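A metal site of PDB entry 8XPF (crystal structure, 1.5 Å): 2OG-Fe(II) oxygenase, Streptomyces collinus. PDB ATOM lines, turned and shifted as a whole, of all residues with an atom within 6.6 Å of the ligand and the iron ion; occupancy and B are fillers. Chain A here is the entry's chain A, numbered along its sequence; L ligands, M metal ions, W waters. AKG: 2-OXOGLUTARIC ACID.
The iron ion is bound by OD2 of Asp 115 (2.0 Å), water W1 (2.1 Å), O5 of the ligand (2.1 Å), NE2 of His 203 (2.2 Å), NE2 of His 113 (2.2 Å) and O1 of the ligand (2.2 Å).
Water W5 bridges O of Gly 136 (3.0 Å) and O2 of the ligand (3.4 Å).
An oxygen (O4) of the ligand sits at hydrogen-bond distance from the side-chain hydroxyl (OG1) of Thr 150, 2.6 Å away.
An oxygen (O3) of the ligand lies within salt-bridge range of the guanidinium group (NH2) of Arg 215.
O5 of the ligand lies close to OE1 of Gln 110.
Three residues have an atom within 4 Å of the iron ion: His 113, Asp 115 and His 203.
The nearest printed residue that does not touch the iron ion is Gln 110 (4.8 Å).
O of Asp 115 lies close to OH of Tyr 135.
The side-chain hydroxyl (OH) of Tyr 139 lies within hydrogen-bond range of the side-chain hydroxyl (OG1) of Thr 150 (2.8 Å).
The backbone NH of Arg 215 sits at hydrogen-bond distance from the backbone carbonyl oxygen of Lys 99 (2.8 Å).
The backbone carbonyl oxygen (O) of Ala 148 sits at hydrogen-bond distance from the guanidinium group (NH1) of Arg 215, at 2.9 Å.
The backbone NH (N) of Gly 205 is in hydrogen-bond range of the side-chain amide oxygen (OE1) of Gln 110 (2.9 Å).
The backbone NH (N) of Tyr 135 is in hydrogen-bond range of the backbone carbonyl oxygen (O) of Phe 197 (2.8 Å).
N of Ile 137 sits at hydrogen-bond distance from O of Leu 195 (2.8 Å).
The backbone carbonyl oxygen of Phe 95 lies within hydrogen-bond range of the backbone NH of Phe 219 (2.8 Å).
Ile 137 touches the ligand.
Phe 197 touches the ligand (CZ to O1, 3.6 Å).
N of Gly 205 touches C4 of the ligand (3.7 Å).
Phe 219 touches the ligand.
Hydrophobic or aromatic side chains within 4 Å of the ligand: His 113, Ile 137, Phe 197, His 203 and Phe 219.
Of the 23 residues printed, 10 come within 4 Å of the ligand.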
ATOM      1  N   PHE A  95     -10.776  -2.648 -33.710  1.00  0.00           N
ATOM      2  CA  PHE A  95     -10.101  -3.936 -33.672  1.00  0.00           C
ATOM      3  C   PHE A  95     -11.147  -5.027 -33.533  1.00  0.00           C
ATOM      4  O   PHE A  95     -12.302  -4.751 -33.188  1.00  0.00           O
ATOM      5  CB  PHE A  95      -9.063  -4.020 -32.525  1.00  0.00           C
ATOM      6  CG  PHE A  95      -9.654  -3.815 -31.152  1.00  0.00           C
ATOM      7  CD1 PHE A  95     -10.095  -4.911 -30.421  1.00  0.00           C
ATOM      8  CD2 PHE A  95      -9.732  -2.555 -30.582  1.00  0.00           C
ATOM      9  CE1 PHE A  95     -10.623  -4.740 -29.131  1.00  0.00           C
ATOM     10  CE2 PHE A  95     -10.281  -2.373 -29.298  1.00  0.00           C
ATOM     11  CZ  PHE A  95     -10.711  -3.480 -28.593  1.00  0.00           C
ATOM     12  N   GLN A  97     -11.707  -8.965 -31.710  1.00  0.00           N
ATOM     13  CA  GLN A  97     -11.129  -9.803 -30.675  1.00  0.00           C
ATOM     14  C   GLN A  97     -12.058 -10.961 -30.370  1.00  0.00           C
ATOM     15  O   GLN A  97     -13.290 -10.837 -30.448  1.00  0.00           O
ATOM     16  CB  GLN A  97     -10.858  -9.007 -29.386  1.00  0.00           C
ATOM     17  CG  GLN A  97      -9.925  -9.725 -28.392  1.00  0.00           C
ATOM     18  CD  GLN A  97      -9.526  -8.840 -27.223  1.00  0.00           C
ATOM     19  OE1 GLN A  97     -10.341  -8.081 -26.675  1.00  0.00           O
ATOM     20  NE2 GLN A  97      -8.259  -8.960 -26.801  1.00  0.00           N
ATOM     21  N   LYS A  99     -12.780 -13.796 -27.255  1.00  0.00           N
ATOM     22  CA  LYS A  99     -12.535 -14.122 -25.860  1.00  0.00           C
ATOM     23  C   LYS A  99     -12.942 -15.575 -25.642  1.00  0.00           C
ATOM     24  O   LYS A  99     -14.110 -15.929 -25.823  1.00  0.00           O
ATOM     25  CB  LYS A  99     -13.326 -13.208 -24.923  1.00  0.00           C
ATOM     26  CG  LYS A  99     -12.936 -13.391 -23.483  1.00  0.00           C
ATOM     27  CD  LYS A  99     -13.630 -12.398 -22.592  1.00  0.00           C
ATOM     28  CE  LYS A  99     -13.008 -11.032 -22.692  1.00  0.00           C
ATOM     29  NZ  LYS A  99     -13.449 -10.169 -21.545  1.00  0.00           N
ATOM     30  N   GLN A 110     -11.791  -8.006 -15.967  1.00  0.00           N
ATOM     31  CA  GLN A 110     -11.143  -6.709 -15.870  1.00  0.00           C
ATOM     32  C   GLN A 110     -11.680  -5.972 -14.642  1.00  0.00           C
ATOM     33  O   GLN A 110     -12.780  -6.236 -14.162  1.00  0.00           O
ATOM     34  CB  GLN A 110     -11.500  -5.853 -17.084  1.00  0.00           C
ATOM     35  CG  GLN A 110     -10.951  -6.306 -18.423  1.00  0.00           C
ATOM     36  CD  GLN A 110     -11.288  -5.323 -19.559  1.00  0.00           C
ATOM     37  OE1 GLN A 110     -12.262  -4.577 -19.492  1.00  0.00           O
ATOM     38  NE2 GLN A 110     -10.471  -5.339 -20.604  1.00  0.00           N
ATOM     39  N   HIS A 113     -13.616   0.418 -14.941  1.00  0.00           N
ATOM     40  CA  HIS A 113     -12.770   1.530 -15.376  1.00  0.00           C
ATOM     41  C   HIS A 113     -13.599   2.441 -16.274  1.00  0.00           C
ATOM     42  O   HIS A 113     -14.705   2.094 -16.698  1.00  0.00           O
ATOM     43  CB  HIS A 113     -11.553   1.005 -16.152  1.00  0.00           C
ATOM     44  CG  HIS A 113     -11.904   0.299 -17.427  1.00  0.00           C
ATOM     45  ND1 HIS A 113     -12.208  -1.051 -17.460  1.00  0.00           N
ATOM     46  CD2 HIS A 113     -12.016   0.749 -18.697  1.00  0.00           C
ATOM     47  CE1 HIS A 113     -12.478  -1.399 -18.707  1.00  0.00           C
ATOM     48  NE2 HIS A 113     -12.387  -0.327 -19.472  1.00  0.00           N
ATOM     49  N   ASN A 114     -13.048   3.623 -16.544  1.00  0.00           N
ATOM     50  CA  ASN A 114     -13.550   4.466 -17.614  1.00  0.00           C
ATOM     51  C   ASN A 114     -12.548   4.466 -18.764  1.00  0.00           C
ATOM     52  O   ASN A 114     -11.379   4.120 -18.601  1.00  0.00           O
ATOM     53  CB  ASN A 114     -13.832   5.913 -17.143  1.00  0.00           C
ATOM     54  CG  ASN A 114     -12.559   6.716 -16.880  1.00  0.00           C
ATOM     55  OD1 ASN A 114     -11.855   7.112 -17.810  1.00  0.00           O
ATOM     56  ND2 ASN A 114     -12.257   6.960 -15.613  1.00  0.00           N
ATOM     57  N   ASP A 115     -13.069   4.805 -19.939  1.00  0.00           N
ATOM     58  CA  ASP A 115     -12.217   4.976 -21.123  1.00  0.00           C
ATOM     59  C   ASP A 115     -12.373   6.401 -21.613  1.00  0.00           C
ATOM     60  O   ASP A 115     -12.621   6.661 -22.797  1.00  0.00           O
ATOM     61  CB  ASP A 115     -12.601   3.970 -22.216  1.00  0.00           C
ATOM     62  CG  ASP A 115     -12.107   2.577 -21.929  1.00  0.00           C
ATOM     63  OD1 ASP A 115     -10.867   2.369 -21.891  1.00  0.00           O
ATOM     64  OD2 ASP A 115     -12.940   1.677 -21.721  1.00  0.00           O
ATOM     65  N   TYR A 135     -17.864   4.643 -27.739  1.00  0.00           N
ATOM     66  CA  TYR A 135     -17.372   3.288 -27.976  1.00  0.00           C
ATOM     67  C   TYR A 135     -18.486   2.426 -28.530  1.00  0.00           C
ATOM     68  O   TYR A 135     -19.654   2.589 -28.160  1.00  0.00           O
ATOM     69  CB  TYR A 135     -16.887   2.651 -26.656  1.00  0.00           C
ATOM     70  CG  TYR A 135     -15.523   3.151 -26.272  1.00  0.00           C
ATOM     71  CD1 TYR A 135     -15.344   4.455 -25.838  1.00  0.00           C
ATOM     72  CD2 TYR A 135     -14.413   2.324 -26.379  1.00  0.00           C
ATOM     73  CE1 TYR A 135     -14.084   4.927 -25.518  1.00  0.00           C
ATOM     74  CE2 TYR A 135     -13.157   2.785 -26.051  1.00  0.00           C
ATOM     75  CZ  TYR A 135     -13.006   4.085 -25.623  1.00  0.00           C
ATOM     76  OH  TYR A 135     -11.744   4.510 -25.319  1.00  0.00           O
ATOM     77  N   GLY A 136     -18.130   1.515 -29.414  1.00  0.00           N
ATOM     78  CA  GLY A 136     -19.077   0.513 -29.884  1.00  0.00           C
ATOM     79  C   GLY A 136     -18.483  -0.882 -29.757  1.00  0.00           C
ATOM     80  O   GLY A 136     -17.290  -1.081 -29.985  1.00  0.00           O
ATOM     81  N   ILE A 137     -19.333  -1.839 -29.422  1.00  0.00           N
ATOM     82  CA  ILE A 137     -18.999  -3.253 -29.498  1.00  0.00           C
ATOM     83  C   ILE A 137     -20.099  -3.916 -30.299  1.00  0.00           C
ATOM     84  O   ILE A 137     -21.253  -3.939 -29.882  1.00  0.00           O
ATOM     85  CB  ILE A 137     -18.886  -3.902 -28.117  1.00  0.00           C
ATOM     86  CG1 ILE A 137     -17.931  -3.106 -27.233  1.00  0.00           C
ATOM     87  CG2 ILE A 137     -18.390  -5.326 -28.272  1.00  0.00           C
ATOM     88  CD1 ILE A 137     -17.789  -3.665 -25.812  1.00  0.00           C
ATOM     89  N   TYR A 139     -21.415  -7.291 -31.419  1.00  0.00           N
ATOM     90  CA  TYR A 139     -21.257  -8.683 -31.034  1.00  0.00           C
ATOM     91  C   TYR A 139     -21.600  -9.566 -32.213  1.00  0.00           C
ATOM     92  O   TYR A 139     -22.666  -9.417 -32.818  1.00  0.00           O
ATOM     93  CB  TYR A 139     -22.190  -9.007 -29.866  1.00  0.00           C
ATOM     94  CG  TYR A 139     -21.939  -8.145 -28.647  1.00  0.00           C
ATOM     95  CD1 TYR A 139     -20.843  -8.378 -27.828  1.00  0.00           C
ATOM     96  CD2 TYR A 139     -22.798  -7.109 -28.325  1.00  0.00           C
ATOM     97  CE1 TYR A 139     -20.615  -7.590 -26.686  1.00  0.00           C
ATOM     98  CE2 TYR A 139     -22.587  -6.331 -27.193  1.00  0.00           C
ATOM     99  CZ  TYR A 139     -21.497  -6.560 -26.398  1.00  0.00           C
ATOM    100  OH  TYR A 139     -21.315  -5.773 -25.267  1.00  0.00           O
ATOM    101  N   ALA A 148     -18.933 -14.092 -21.313  1.00  0.00           N
ATOM    102  CA  ALA A 148     -18.133 -12.880 -21.113  1.00  0.00           C
ATOM    103  C   ALA A 148     -18.885 -11.607 -21.503  1.00  0.00           C
ATOM    104  O   ALA A 148     -18.398 -10.827 -22.331  1.00  0.00           O
ATOM    105  CB  ALA A 148     -16.802 -12.966 -21.871  1.00  0.00           C
ATOM    106  N   PRO A 149     -20.040 -11.353 -20.907  1.00  0.00           N
ATOM    107  CA  PRO A 149     -20.759 -10.112 -21.212  1.00  0.00           C
ATOM    108  C   PRO A 149     -19.996  -8.888 -20.730  1.00  0.00           C
ATOM    109  O   PRO A 149     -19.251  -8.941 -19.742  1.00  0.00           O
ATOM    110  CB  PRO A 149     -22.063 -10.266 -20.426  1.00  0.00           C
ATOM    111  CG  PRO A 149     -21.682 -11.134 -19.271  1.00  0.00           C
ATOM    112  CD  PRO A 149     -20.735 -12.138 -19.877  1.00  0.00           C
ATOM    113  N   THR A 150     -20.184  -7.787 -21.445  1.00  0.00           N
ATOM    114  CA  THR A 150     -19.779  -6.477 -20.945  1.00  0.00           C
ATOM    115  C   THR A 150     -20.616  -6.115 -19.720  1.00  0.00           C
ATOM    116  O   THR A 150     -21.825  -6.362 -19.690  1.00  0.00           O
ATOM    117  CB  THR A 150     -20.038  -5.433 -22.020  1.00  0.00           C
ATOM    118  OG1 THR A 150     -19.436  -5.849 -23.256  1.00  0.00           O
ATOM    119  CG2 THR A 150     -19.427  -4.098 -21.630  1.00  0.00           C
ATOM    120  N   TYR A 151     -19.974  -5.556 -18.697  1.00  0.00           N
ATOM    121  CA  TYR A 151     -20.681  -5.014 -17.536  1.00  0.00           C
ATOM    122  C   TYR A 151     -20.654  -3.496 -17.586  1.00  0.00           C
ATOM    123  O   TYR A 151     -19.644  -2.892 -17.967  1.00  0.00           O
ATOM    124  CB  TYR A 151     -20.058  -5.477 -16.221  1.00  0.00           C
ATOM    125  CG  TYR A 151     -20.487  -6.847 -15.740  1.00  0.00           C
ATOM    126  CD1 TYR A 151     -20.015  -7.996 -16.371  1.00  0.00           C
ATOM    127  CD2 TYR A 151     -21.354  -6.983 -14.666  1.00  0.00           C
ATOM    128  CE1 TYR A 151     -20.397  -9.254 -15.936  1.00  0.00           C
ATOM    129  CE2 TYR A 151     -21.740  -8.232 -14.233  1.00  0.00           C
ATOM    130  CZ  TYR A 151     -21.255  -9.354 -14.872  1.00  0.00           C
ATOM    131  OH  TYR A 151     -21.651 -10.591 -14.414  1.00  0.00           O
ATOM    132  N   LEU A 195     -23.564  -2.577 -28.887  1.00  0.00           N
ATOM    133  CA  LEU A 195     -23.559  -1.804 -27.656  1.00  0.00           C
ATOM    134  C   LEU A 195     -22.798  -0.514 -27.927  1.00  0.00           C
ATOM    135  O   LEU A 195     -21.632  -0.557 -28.356  1.00  0.00           O
ATOM    136  CB  LEU A 195     -22.895  -2.566 -26.507  1.00  0.00           C
ATOM    137  CG  LEU A 195     -22.791  -1.776 -25.205  1.00  0.00           C
ATOM    138  CD1 LEU A 195     -24.172  -1.528 -24.623  1.00  0.00           C
ATOM    139  CD2 LEU A 195     -21.903  -2.522 -24.196  1.00  0.00           C
ATOM    140  N   PHE A 197     -21.517   3.052 -25.984  1.00  0.00           N
ATOM    141  CA  PHE A 197     -21.358   3.646 -24.667  1.00  0.00           C
ATOM    142  C   PHE A 197     -20.419   4.842 -24.718  1.00  0.00           C
ATOM    143  O   PHE A 197     -19.586   4.967 -25.616  1.00  0.00           O
ATOM    144  CB  PHE A 197     -20.959   2.623 -23.585  1.00  0.00           C
ATOM    145  CG  PHE A 197     -19.624   1.955 -23.791  1.00  0.00           C
ATOM    146  CD1 PHE A 197     -18.466   2.489 -23.238  1.00  0.00           C
ATOM    147  CD2 PHE A 197     -19.543   0.733 -24.445  1.00  0.00           C
ATOM    148  CE1 PHE A 197     -17.253   1.836 -23.379  1.00  0.00           C
ATOM    149  CE2 PHE A 197     -18.332   0.087 -24.601  1.00  0.00           C
ATOM    150  CZ  PHE A 197     -17.198   0.622 -24.047  1.00  0.00           C
ATOM    151  N   HIS A 203     -17.366   0.705 -16.529  1.00  0.00           N
ATOM    152  CA  HIS A 203     -17.724  -0.531 -17.194  1.00  0.00           C
ATOM    153  C   HIS A 203     -16.517  -1.466 -17.128  1.00  0.00           C
ATOM    154  O   HIS A 203     -15.417  -1.063 -16.741  1.00  0.00           O
ATOM    155  CB  HIS A 203     -18.082  -0.273 -18.666  1.00  0.00           C
ATOM    156  CG  HIS A 203     -16.898   0.159 -19.468  1.00  0.00           C
ATOM    157  ND1 HIS A 203     -16.407   1.445 -19.450  1.00  0.00           N
ATOM    158  CD2 HIS A 203     -16.058  -0.545 -20.273  1.00  0.00           C
ATOM    159  CE1 HIS A 203     -15.341   1.526 -20.223  1.00  0.00           C
ATOM    160  NE2 HIS A 203     -15.098   0.325 -20.718  1.00  0.00           N
ATOM    161  N   ARG A 204     -16.725  -2.707 -17.575  1.00  0.00           N
ATOM    162  CA  ARG A 204     -15.612  -3.642 -17.669  1.00  0.00           C
ATOM    163  C   ARG A 204     -16.002  -4.792 -18.585  1.00  0.00           C
ATOM    164  O   ARG A 204     -17.181  -5.086 -18.777  1.00  0.00           O
ATOM    165  CB  ARG A 204     -15.228  -4.204 -16.302  1.00  0.00           C
ATOM    166  CG  ARG A 204     -16.303  -5.085 -15.669  1.00  0.00           C
ATOM    167  CD  ARG A 204     -15.835  -5.634 -14.321  1.00  0.00           C
ATOM    168  NE  ARG A 204     -16.846  -6.458 -13.666  1.00  0.00           N
ATOM    169  CZ  ARG A 204     -16.938  -7.773 -13.830  1.00  0.00           C
ATOM    170  NH1 ARG A 204     -16.101  -8.429 -14.618  1.00  0.00           N
ATOM    171  NH2 ARG A 204     -17.890  -8.438 -13.187  1.00  0.00           N
ATOM    172  N   GLY A 205     -14.985  -5.458 -19.135  1.00  0.00           N
ATOM    173  CA  GLY A 205     -15.164  -6.808 -19.621  1.00  0.00           C
ATOM    174  C   GLY A 205     -15.187  -7.808 -18.478  1.00  0.00           C
ATOM    175  O   GLY A 205     -14.847  -7.505 -17.326  1.00  0.00           O
ATOM    176  N   SER A 206     -15.623  -9.023 -18.791  1.00  0.00           N
ATOM    177  CA  SER A 206     -15.782 -10.047 -17.771  1.00  0.00           C
ATOM    178  C   SER A 206     -15.203 -11.369 -18.240  1.00  0.00           C
ATOM    179  O   SER A 206     -14.909 -11.575 -19.411  1.00  0.00           O
ATOM    180  CB  SER A 206     -17.248 -10.207 -17.328  1.00  0.00           C
ATOM    181  OG  SER A 206     -18.034 -10.811 -18.357  1.00  0.00           O
ATOM    182  N   ARG A 215     -16.349 -15.753 -27.504  1.00  0.00           N
ATOM    183  CA  ARG A 215     -17.119 -14.576 -27.887  1.00  0.00           C
ATOM    184  C   ARG A 215     -16.383 -13.859 -29.008  1.00  0.00           C
ATOM    185  O   ARG A 215     -15.167 -13.664 -28.928  1.00  0.00           O
ATOM    186  CB  ARG A 215     -17.279 -13.619 -26.701  1.00  0.00           C
ATOM    187  CG  ARG A 215     -18.239 -12.475 -26.991  1.00  0.00           C
ATOM    188  CD  ARG A 215     -18.235 -11.396 -25.899  1.00  0.00           C
ATOM    189  NE  ARG A 215     -17.059 -10.550 -25.993  1.00  0.00           N
ATOM    190  CZ  ARG A 215     -16.890  -9.421 -25.315  1.00  0.00           C
ATOM    191  NH1 ARG A 215     -17.817  -8.985 -24.477  1.00  0.00           N
ATOM    192  NH2 ARG A 215     -15.787  -8.717 -25.496  1.00  0.00           N
ATOM    193  N   PHE A 219     -14.803  -4.042 -32.261  1.00  0.00           N
ATOM    194  CA  PHE A 219     -14.762  -2.910 -31.357  1.00  0.00           C
ATOM    195  C   PHE A 219     -14.356  -1.676 -32.148  1.00  0.00           C
ATOM    196  O   PHE A 219     -13.578  -1.777 -33.090  1.00  0.00           O
ATOM    197  CB  PHE A 219     -13.679  -3.118 -30.302  1.00  0.00           C
ATOM    198  CG  PHE A 219     -13.940  -4.269 -29.386  1.00  0.00           C
ATOM    199  CD1 PHE A 219     -13.760  -5.567 -29.832  1.00  0.00           C
ATOM    200  CD2 PHE A 219     -14.298  -4.048 -28.070  1.00  0.00           C
ATOM    201  CE1 PHE A 219     -13.976  -6.643 -28.980  1.00  0.00           C
ATOM    202  CE2 PHE A 219     -14.513  -5.111 -27.211  1.00  0.00           C
ATOM    203  CZ  PHE A 219     -14.338  -6.414 -27.666  1.00  0.00           C
HETATM  204  C1  AKG L   1     -14.163  -1.669 -23.758  1.00  0.00           C
HETATM  205  O1  AKG L   1     -13.849  -0.490 -23.556  1.00  0.00           O
HETATM  206  O2  AKG L   1     -14.624  -2.129 -24.911  1.00  0.00           O
HETATM  207  C2  AKG L   1     -13.996  -2.735 -22.643  1.00  0.00           C
HETATM  208  O5  AKG L   1     -13.697  -2.356 -21.517  1.00  0.00           O
HETATM  209  C3  AKG L   1     -14.152  -4.191 -23.002  1.00  0.00           C
HETATM  210  C4  AKG L   1     -15.530  -4.742 -22.683  1.00  0.00           C
HETATM  211  C5  AKG L   1     -15.757  -6.131 -23.248  1.00  0.00           C
HETATM  212  O3  AKG L   1     -14.897  -6.756 -23.839  1.00  0.00           O
HETATM  213  O4  AKG L   1     -16.953  -6.591 -23.044  1.00  0.00           O
HETATM  214 FE    FE M   1     -13.183  -0.271 -21.494  1.00  0.00          FE
HETATM  215  O   HOH W   1     -11.276  -0.689 -22.314  1.00  0.00           O
HETATM  216  O   HOH W   2     -11.517  -3.261 -25.014  1.00  0.00           O
HETATM  217  O   HOH W   3     -16.193  -9.158 -21.673  1.00  0.00           O
HETATM  218  O   HOH W   4     -11.781  -0.549 -26.105  1.00  0.00           O
HETATM  219  O   HOH W   5     -15.292  -0.591 -27.848  1.00  0.00           O
